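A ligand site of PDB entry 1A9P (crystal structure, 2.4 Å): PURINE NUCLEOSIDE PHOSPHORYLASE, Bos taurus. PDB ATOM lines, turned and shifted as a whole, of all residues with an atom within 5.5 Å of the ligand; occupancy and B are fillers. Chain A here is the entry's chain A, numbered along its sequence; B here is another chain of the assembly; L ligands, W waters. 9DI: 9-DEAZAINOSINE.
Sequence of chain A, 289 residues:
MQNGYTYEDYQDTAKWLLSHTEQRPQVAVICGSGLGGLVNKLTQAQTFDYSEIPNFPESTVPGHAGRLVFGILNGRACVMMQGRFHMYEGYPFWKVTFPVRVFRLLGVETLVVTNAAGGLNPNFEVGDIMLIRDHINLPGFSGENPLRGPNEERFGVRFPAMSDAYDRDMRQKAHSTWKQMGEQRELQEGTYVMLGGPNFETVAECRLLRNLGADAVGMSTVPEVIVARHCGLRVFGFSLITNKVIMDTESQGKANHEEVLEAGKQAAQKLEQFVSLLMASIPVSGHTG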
ATOM      1  N   SER A  33       7.937 -14.540   2.698  1.00  0.00           N
ATOM      2  CA  SER A  33       8.127 -13.135   2.366  1.00  0.00           C
ATOM      3  C   SER A  33       6.909 -12.282   2.706  1.00  0.00           C
ATOM      4  O   SER A  33       5.781 -12.618   2.355  1.00  0.00           O
ATOM      5  CB  SER A  33       8.471 -12.979   0.885  1.00  0.00           C
ATOM      6  OG  SER A  33       9.813 -13.329   0.627  1.00  0.00           O
ATOM      7  N   VAL A  61      17.313 -12.454   3.276  1.00  0.00           N
ATOM      8  CA  VAL A  61      16.320 -11.855   2.400  1.00  0.00           C
ATOM      9  C   VAL A  61      15.437 -10.820   3.095  1.00  0.00           C
ATOM     10  O   VAL A  61      14.936 -11.064   4.201  1.00  0.00           O
ATOM     11  CB  VAL A  61      15.396 -12.975   1.792  1.00  0.00           C
ATOM     12  CG1 VAL A  61      14.254 -12.368   0.968  1.00  0.00           C
ATOM     13  CG2 VAL A  61      16.214 -13.922   0.931  1.00  0.00           C
ATOM     14  N   HIS A  64      12.335 -11.171   5.649  1.00  0.00           N
ATOM     15  CA  HIS A  64      12.617 -12.289   6.524  1.00  0.00           C
ATOM     16  C   HIS A  64      13.489 -11.739   7.662  1.00  0.00           C
ATOM     17  O   HIS A  64      14.687 -11.525   7.495  1.00  0.00           O
ATOM     18  CB  HIS A  64      13.337 -13.407   5.748  1.00  0.00           C
ATOM     19  CG  HIS A  64      12.492 -14.059   4.694  1.00  0.00           C
ATOM     20  ND1 HIS A  64      12.332 -13.516   3.436  1.00  0.00           N
ATOM     21  CD2 HIS A  64      11.729 -15.181   4.723  1.00  0.00           C
ATOM     22  CE1 HIS A  64      11.507 -14.276   2.730  1.00  0.00           C
ATOM     23  NE2 HIS A  64      11.130 -15.288   3.486  1.00  0.00           N
ATOM     24  N   HIS A  86      16.312 -19.937   1.940  1.00  0.00           N
ATOM     25  CA  HIS A  86      16.066 -20.389   0.588  1.00  0.00           C
ATOM     26  C   HIS A  86      17.371 -20.907  -0.025  1.00  0.00           C
ATOM     27  O   HIS A  86      18.461 -20.496   0.369  1.00  0.00           O
ATOM     28  CB  HIS A  86      15.530 -19.243  -0.275  1.00  0.00           C
ATOM     29  CG  HIS A  86      14.299 -18.574   0.273  1.00  0.00           C
ATOM     30  ND1 HIS A  86      14.352 -17.619   1.264  1.00  0.00           N
ATOM     31  CD2 HIS A  86      13.001 -18.681  -0.084  1.00  0.00           C
ATOM     32  CE1 HIS A  86      13.136 -17.159   1.487  1.00  0.00           C
ATOM     33  NE2 HIS A  86      12.292 -17.784   0.681  1.00  0.00           N
ATOM     34  N   TYR A  88      18.348 -20.243  -3.039  1.00  0.00           N
ATOM     35  CA  TYR A  88      18.978 -19.157  -3.813  1.00  0.00           C
ATOM     36  C   TYR A  88      19.898 -18.265  -2.984  1.00  0.00           C
ATOM     37  O   TYR A  88      20.517 -17.367  -3.530  1.00  0.00           O
ATOM     38  CB  TYR A  88      17.944 -18.285  -4.567  1.00  0.00           C
ATOM     39  CG  TYR A  88      16.949 -17.505  -3.727  1.00  0.00           C
ATOM     40  CD1 TYR A  88      17.351 -16.419  -2.945  1.00  0.00           C
ATOM     41  CD2 TYR A  88      15.590 -17.848  -3.718  1.00  0.00           C
ATOM     42  CE1 TYR A  88      16.447 -15.702  -2.171  1.00  0.00           C
ATOM     43  CE2 TYR A  88      14.681 -17.140  -2.945  1.00  0.00           C
ATOM     44  CZ  TYR A  88      15.106 -16.070  -2.177  1.00  0.00           C
ATOM     45  OH  TYR A  88      14.201 -15.390  -1.398  1.00  0.00           O
ATOM     46  N   ALA A 116       4.918 -16.511  -0.156  1.00  0.00           N
ATOM     47  CA  ALA A 116       4.352 -15.586  -1.119  1.00  0.00           C
ATOM     48  C   ALA A 116       4.603 -16.288  -2.451  1.00  0.00           C
ATOM     49  O   ALA A 116       5.693 -16.816  -2.675  1.00  0.00           O
ATOM     50  CB  ALA A 116       5.105 -14.262  -1.058  1.00  0.00           C
ATOM     51  N   ALA A 117       3.602 -16.311  -3.323  1.00  0.00           N
ATOM     52  CA  ALA A 117       3.769 -16.966  -4.612  1.00  0.00           C
ATOM     53  C   ALA A 117       3.140 -16.215  -5.777  1.00  0.00           C
ATOM     54  O   ALA A 117       2.241 -15.400  -5.598  1.00  0.00           O
ATOM     55  CB  ALA A 117       3.223 -18.381  -4.549  1.00  0.00           C
ATOM     56  N   GLY A 118       3.665 -16.458  -6.973  1.00  0.00           N
ATOM     57  CA  GLY A 118       3.133 -15.839  -8.174  1.00  0.00           C
ATOM     58  C   GLY A 118       1.973 -16.682  -8.644  1.00  0.00           C
ATOM     59  O   GLY A 118       2.015 -17.910  -8.598  1.00  0.00           O
ATOM     60  N   GLY A 119       0.902 -16.024  -9.071  1.00  0.00           N
ATOM     61  CA  GLY A 119      -0.273 -16.754  -9.535  1.00  0.00           C
ATOM     62  C   GLY A 119      -0.156 -17.221 -10.966  1.00  0.00           C
ATOM     63  O   GLY A 119       0.176 -16.440 -11.862  1.00  0.00           O
ATOM     64  N   TYR A 192       1.244 -26.070  -5.713  1.00  0.00           N
ATOM     65  CA  TYR A 192       2.359 -25.150  -5.613  1.00  0.00           C
ATOM     66  C   TYR A 192       3.563 -25.787  -6.296  1.00  0.00           C
ATOM     67  O   TYR A 192       3.863 -26.964  -6.068  1.00  0.00           O
ATOM     68  CB  TYR A 192       2.655 -24.848  -4.134  1.00  0.00           C
ATOM     69  CG  TYR A 192       3.879 -23.997  -3.900  1.00  0.00           C
ATOM     70  CD1 TYR A 192       3.786 -22.605  -3.930  1.00  0.00           C
ATOM     71  CD2 TYR A 192       5.123 -24.581  -3.657  1.00  0.00           C
ATOM     72  CE1 TYR A 192       4.912 -21.816  -3.708  1.00  0.00           C
ATOM     73  CE2 TYR A 192       6.243 -23.799  -3.445  1.00  0.00           C
ATOM     74  CZ  TYR A 192       6.130 -22.418  -3.465  1.00  0.00           C
ATOM     75  OH  TYR A 192       7.245 -21.647  -3.235  1.00  0.00           O
ATOM     76  N   LEU A 195      10.723 -23.788  -7.868  1.00  0.00           N
ATOM     77  CA  LEU A 195      11.882 -23.696  -8.738  1.00  0.00           C
ATOM     78  C   LEU A 195      12.958 -22.998  -7.918  1.00  0.00           C
ATOM     79  O   LEU A 195      12.670 -22.470  -6.851  1.00  0.00           O
ATOM     80  CB  LEU A 195      11.577 -22.963 -10.051  1.00  0.00           C
ATOM     81  CG  LEU A 195      10.541 -21.836 -10.111  1.00  0.00           C
ATOM     82  CD1 LEU A 195      10.968 -20.649  -9.256  1.00  0.00           C
ATOM     83  CD2 LEU A 195      10.384 -21.428 -11.571  1.00  0.00           C
ATOM     84  N   PHE A 200      13.096 -13.939 -11.603  1.00  0.00           N
ATOM     85  CA  PHE A 200      11.704 -14.236 -11.837  1.00  0.00           C
ATOM     86  C   PHE A 200      11.595 -14.941 -13.195  1.00  0.00           C
ATOM     87  O   PHE A 200      12.504 -14.840 -14.026  1.00  0.00           O
ATOM     88  CB  PHE A 200      10.848 -12.978 -11.781  1.00  0.00           C
ATOM     89  CG  PHE A 200      10.590 -12.490 -10.377  1.00  0.00           C
ATOM     90  CD1 PHE A 200       9.864 -13.263  -9.472  1.00  0.00           C
ATOM     91  CD2 PHE A 200      11.074 -11.259  -9.955  1.00  0.00           C
ATOM     92  CE1 PHE A 200       9.620 -12.814  -8.176  1.00  0.00           C
ATOM     93  CE2 PHE A 200      10.828 -10.795  -8.667  1.00  0.00           C
ATOM     94  CZ  PHE A 200      10.103 -11.580  -7.774  1.00  0.00           C
ATOM     95  N   GLU A 201      10.504 -15.659 -13.379  1.00  0.00           N
ATOM     96  CA  GLU A 201      10.266 -16.455 -14.588  1.00  0.00           C
ATOM     97  C   GLU A 201       9.993 -15.685 -15.877  1.00  0.00           C
ATOM     98  O   GLU A 201       9.516 -14.534 -15.862  1.00  0.00           O
ATOM     99  CB  GLU A 201       9.122 -17.446 -14.351  1.00  0.00           C
ATOM    100  CG  GLU A 201       9.255 -18.355 -13.132  1.00  0.00           C
ATOM    101  CD  GLU A 201       9.021 -17.626 -11.818  1.00  0.00           C
ATOM    102  OE1 GLU A 201       8.092 -16.791 -11.754  1.00  0.00           O
ATOM    103  OE2 GLU A 201       9.774 -17.876 -10.844  1.00  0.00           O
ATOM    104  N   VAL A 217       3.610 -20.462  -8.293  1.00  0.00           N
ATOM    105  CA  VAL A 217       5.036 -20.742  -8.364  1.00  0.00           C
ATOM    106  C   VAL A 217       5.817 -19.982  -7.271  1.00  0.00           C
ATOM    107  O   VAL A 217       5.576 -18.791  -7.015  1.00  0.00           O
ATOM    108  CB  VAL A 217       5.577 -20.387  -9.781  1.00  0.00           C
ATOM    109  CG1 VAL A 217       5.197 -18.964 -10.140  1.00  0.00           C
ATOM    110  CG2 VAL A 217       7.084 -20.590  -9.858  1.00  0.00           C
ATOM    111  N   GLY A 218       6.759 -20.660  -6.635  1.00  0.00           N
ATOM    112  CA  GLY A 218       7.540 -20.020  -5.609  1.00  0.00           C
ATOM    113  C   GLY A 218       8.931 -20.596  -5.568  1.00  0.00           C
ATOM    114  O   GLY A 218       9.280 -21.455  -6.392  1.00  0.00           O
ATOM    115  N   MET A 219       9.725 -20.162  -4.602  1.00  0.00           N
ATOM    116  CA  MET A 219      11.103 -20.625  -4.463  1.00  0.00           C
ATOM    117  C   MET A 219      11.393 -21.189  -3.085  1.00  0.00           C
ATOM    118  O   MET A 219      12.524 -21.067  -2.603  1.00  0.00           O
ATOM    119  CB  MET A 219      12.059 -19.440  -4.729  1.00  0.00           C
ATOM    120  CG  MET A 219      11.825 -18.698  -6.036  1.00  0.00           C
ATOM    121  SD  MET A 219      12.819 -17.188  -6.168  1.00  0.00           S
ATOM    122  CE  MET A 219      12.239 -16.456  -7.683  1.00  0.00           C
ATOM    123  N   SER A 220      10.401 -21.813  -2.454  1.00  0.00           N
ATOM    124  CA  SER A 220      10.621 -22.347  -1.107  1.00  0.00           C
ATOM    125  C   SER A 220       9.553 -23.359  -0.707  1.00  0.00           C
ATOM    126  O   SER A 220       8.931 -23.997  -1.551  1.00  0.00           O
ATOM    127  CB  SER A 220      10.604 -21.203  -0.094  1.00  0.00           C
ATOM    128  OG  SER A 220       9.280 -20.746   0.096  1.00  0.00           O
ATOM    129  N   THR A 242       0.805 -12.903  -4.200  1.00  0.00           N
ATOM    130  CA  THR A 242       1.299 -11.542  -4.196  1.00  0.00           C
ATOM    131  C   THR A 242       1.343 -10.868  -5.562  1.00  0.00           C
ATOM    132  O   THR A 242       1.416  -9.646  -5.649  1.00  0.00           O
ATOM    133  CB  THR A 242       2.708 -11.468  -3.569  1.00  0.00           C
ATOM    134  OG1 THR A 242       3.583 -12.385  -4.237  1.00  0.00           O
ATOM    135  CG2 THR A 242       2.641 -11.809  -2.093  1.00  0.00           C
ATOM    136  N   ASN A 243       1.262 -11.656  -6.629  1.00  0.00           N
ATOM    137  CA  ASN A 243       1.324 -11.086  -7.961  1.00  0.00           C
ATOM    138  C   ASN A 243       0.795 -12.040  -9.019  1.00  0.00           C
ATOM    139  O   ASN A 243       0.655 -13.236  -8.782  1.00  0.00           O
ATOM    140  CB  ASN A 243       2.778 -10.734  -8.320  1.00  0.00           C
ATOM    141  CG  ASN A 243       3.711 -11.955  -8.306  1.00  0.00           C
ATOM    142  OD1 ASN A 243       4.076 -12.461  -7.250  1.00  0.00           O
ATOM    143  ND2 ASN A 243       4.105 -12.415  -9.483  1.00  0.00           N
ATOM    144  N   VAL A 245       1.614 -13.633 -12.573  1.00  0.00           N
ATOM    145  CA  VAL A 245       2.786 -13.819 -13.413  1.00  0.00           C
ATOM    146  C   VAL A 245       2.519 -13.381 -14.840  1.00  0.00           C
ATOM    147  O   VAL A 245       1.376 -13.417 -15.330  1.00  0.00           O
ATOM    148  CB  VAL A 245       3.308 -15.268 -13.421  1.00  0.00           C
ATOM    149  CG1 VAL A 245       3.660 -15.706 -12.010  1.00  0.00           C
ATOM    150  CG2 VAL A 245       2.297 -16.207 -14.068  1.00  0.00           C
ATOM    151  N   ALA A 255       7.786  -8.434 -12.873  1.00  0.00           N
ATOM    152  CA  ALA A 255       7.724  -8.724 -11.442  1.00  0.00           C
ATOM    153  C   ALA A 255       8.902  -8.108 -10.701  1.00  0.00           C
ATOM    154  O   ALA A 255       9.970  -7.886 -11.273  1.00  0.00           O
ATOM    155  CB  ALA A 255       7.690 -10.251 -11.209  1.00  0.00           C
ATOM    156  N   ASN A 256       8.688  -7.817  -9.429  1.00  0.00           N
ATOM    157  CA  ASN A 256       9.720  -7.239  -8.572  1.00  0.00           C
ATOM    158  C   ASN A 256       9.423  -7.579  -7.120  1.00  0.00           C
ATOM    159  O   ASN A 256       8.289  -7.922  -6.763  1.00  0.00           O
ATOM    160  CB  ASN A 256       9.813  -5.720  -8.790  1.00  0.00           C
ATOM    161  CG  ASN A 256       8.501  -4.998  -8.573  1.00  0.00           C
ATOM    162  OD1 ASN A 256       8.105  -4.733  -7.444  1.00  0.00           O
ATOM    163  ND2 ASN A 256       7.817  -4.675  -9.673  1.00  0.00           N
ATOM    164  N   HIS A 257      10.439  -7.479  -6.268  1.00  0.00           N
ATOM    165  CA  HIS A 257      10.289  -7.814  -4.857  1.00  0.00           C
ATOM    166  C   HIS A 257       9.303  -6.923  -4.073  1.00  0.00           C
ATOM    167  O   HIS A 257       8.968  -7.258  -2.932  1.00  0.00           O
ATOM    168  CB  HIS A 257      11.651  -7.872  -4.164  1.00  0.00           C
ATOM    169  CG  HIS A 257      11.649  -8.623  -2.872  1.00  0.00           C
ATOM    170  ND1 HIS A 257      10.961  -9.813  -2.707  1.00  0.00           N
ATOM    171  CD2 HIS A 257      12.244  -8.360  -1.673  1.00  0.00           C
ATOM    172  CE1 HIS A 257      11.140 -10.257  -1.466  1.00  0.00           C
ATOM    173  NE2 HIS A 257      11.911  -9.387  -0.822  1.00  0.00           N
ATOM    174  N   GLU A 259       6.495  -7.019  -3.985  1.00  0.00           N
ATOM    175  CA  GLU A 259       5.372  -7.871  -3.639  1.00  0.00           C
ATOM    176  C   GLU A 259       5.175  -7.992  -2.113  1.00  0.00           C
ATOM    177  O   GLU A 259       4.168  -8.528  -1.650  1.00  0.00           O
ATOM    178  CB  GLU A 259       5.521  -9.247  -4.289  1.00  0.00           C
ATOM    179  CG  GLU A 259       6.858  -9.937  -4.068  1.00  0.00           C
ATOM    180  CD  GLU A 259       6.955 -10.605  -2.711  1.00  0.00           C
ATOM    181  OE1 GLU A 259       6.162 -11.548  -2.463  1.00  0.00           O
ATOM    182  OE2 GLU A 259       7.818 -10.209  -1.908  1.00  0.00           O
ATOM    183  N   PHE B 159      16.297  -9.892  -6.748  1.00  0.00           N
ATOM    184  CA  PHE B 159      15.291 -10.541  -7.587  1.00  0.00           C
ATOM    185  C   PHE B 159      15.069  -9.844  -8.921  1.00  0.00           C
ATOM    186  O   PHE B 159      14.074  -9.129  -9.082  1.00  0.00           O
ATOM    187  CB  PHE B 159      13.950 -10.609  -6.852  1.00  0.00           C
ATOM    188  CG  PHE B 159      14.008 -11.319  -5.539  1.00  0.00           C
ATOM    189  CD1 PHE B 159      14.108 -12.705  -5.498  1.00  0.00           C
ATOM    190  CD2 PHE B 159      13.956 -10.604  -4.351  1.00  0.00           C
ATOM    191  CE1 PHE B 159      14.183 -13.369  -4.281  1.00  0.00           C
ATOM    192  CE2 PHE B 159      14.023 -11.262  -3.132  1.00  0.00           C
ATOM    193  CZ  PHE B 159      14.129 -12.639  -3.091  1.00  0.00           C
HETATM  194  C9  9DI L   1       7.678 -15.205  -4.950  1.00  0.00           C
HETATM  195  C4  9DI L   1       7.886 -15.705  -6.230  1.00  0.00           C
HETATM  196  N3  9DI L   1       8.780 -16.629  -6.689  1.00  0.00           N
HETATM  197  C2  9DI L   1       8.658 -16.850  -8.017  1.00  0.00           C
HETATM  198  N1  9DI L   1       7.751 -16.220  -8.824  1.00  0.00           N
HETATM  199  C6  9DI L   1       6.845 -15.271  -8.392  1.00  0.00           C
HETATM  200  O6  9DI L   1       6.080 -14.736  -9.203  1.00  0.00           O
HETATM  201  C5  9DI L   1       6.939 -15.024  -6.977  1.00  0.00           C
HETATM  202  N7  9DI L   1       6.199 -14.156  -6.194  1.00  0.00           N
HETATM  203  C8  9DI L   1       6.670 -14.284  -4.910  1.00  0.00           C
HETATM  204  C5' 9DI L   1      10.493 -12.974  -4.060  1.00  0.00           C
HETATM  205  O5' 9DI L   1       9.534 -11.900  -3.890  1.00  0.00           O
HETATM  206  C4' 9DI L   1      10.238 -14.028  -3.005  1.00  0.00           C
HETATM  207  O4' 9DI L   1       8.813 -14.300  -3.103  1.00  0.00           O
HETATM  208  C1' 9DI L   1       8.494 -15.542  -3.680  1.00  0.00           C
HETATM  209  C2' 9DI L   1       9.866 -16.233  -3.907  1.00  0.00           C
HETATM  210  O2' 9DI L   1       9.870 -17.606  -3.463  1.00  0.00           O
HETATM  211  C3' 9DI L   1      10.964 -15.347  -3.254  1.00  0.00           C
HETATM  212  O3' 9DI L   1      11.518 -15.860  -2.019  1.00  0.00           O
HETATM  213  O   HOH W   1       7.209 -19.099  -2.306  1.00  0.00           O
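The backbone NH of Met 219 sits at hydrogen-bond distance from an oxygen (O2') of the ligand (2.8 Å).
The side-chain carboxylate of Glu 201 is in hydrogen-bond range of a nitrogen (N1) of the ligand (3.0 Å).
An oxygen (O3') of the ligand sits at hydrogen-bond distance from the side-chain hydroxyl (OH) of Tyr 88.
NE2 of His 86 is in hydrogen-bond range of O3' of the ligand (3.4 Å).
The side-chain amide oxygen of Asn 243 is in hydrogen-bond range of a nitrogen (N7) of the ligand, at 2.9 Å.
An oxygen (O5') of the ligand sits close to the side-chain carboxylate (OE2) of Glu 259 (3.1 Å).
ND1 of His 257 is in hydrogen-bond range of O5' of the ligand (2.8 Å).
A ring nitrogen (NE2) of His 64 is in hydrogen-bond range of the backbone NH (N) of Ser 33, at 3.4 Å.
N of Met 219 lies within hydrogen-bond range of OH of Tyr 192 (3.2 Å).
A ring nitrogen (ND1) of His 86 lies within hydrogen-bond range of the side-chain hydroxyl of Tyr 88, at 3.5 Å.
The backbone carbonyl oxygen of Gly 119 lies close to the backbone NH of Val 245, at 3.2 Å.
The backbone NH (N) of Gly 119 is in hydrogen-bond range of the backbone carbonyl oxygen (O) of Asn 243 (2.8 Å).
The backbone carbonyl oxygen (O) of Gly 218 is in hydrogen-bond range of the backbone NH (N) of Leu 195, at 3.1 Å.
The side-chain hydroxyl (OG1) of Thr 242 lies within hydrogen-bond range of the side-chain carboxylate (OE1) of Glu 259, at 3.2 Å.
The backbone NH (N) of Thr 242 lies within hydrogen-bond range of the backbone carbonyl oxygen (O) of Ala 117.
Merely in contact with the ligand: Ala 116 (3.2 Å), Gly 118 (3.3 Å), Phe 200 (3.7 Å), Thr 242 (3.7 Å), Ala 117 (3.7 Å), Phe 159 of chain B (3.7 Å), Ser 33 (3.7 Å), Gly 218 (3.8 Å), Val 217 (3.8 Å) and Val 245 (3.8 Å).
Hydrophobic or aromatic side chains that line the ligand: His 86, Tyr 88, Phe 200, Val 217, Met 219, Val 245, His 257 and Phe 159 of chain B.
17 residues have an atom within 4 Å of the ligand: Ser 33, His 86, Tyr 88, Ala 116, Ala 117, Gly 118, Phe 200, Glu 201, Val 217, Gly 218, Met 219, Thr 242, Asn 243, Val 245, His 257, Glu 259 and Phe 159 of chain B.
Water W1 lies within hydrogen-bond range of OH of Tyr 192 (2.7 Å), O of Ala 116 (2.8 Å) and O2' of the ligand (3.3 Å).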
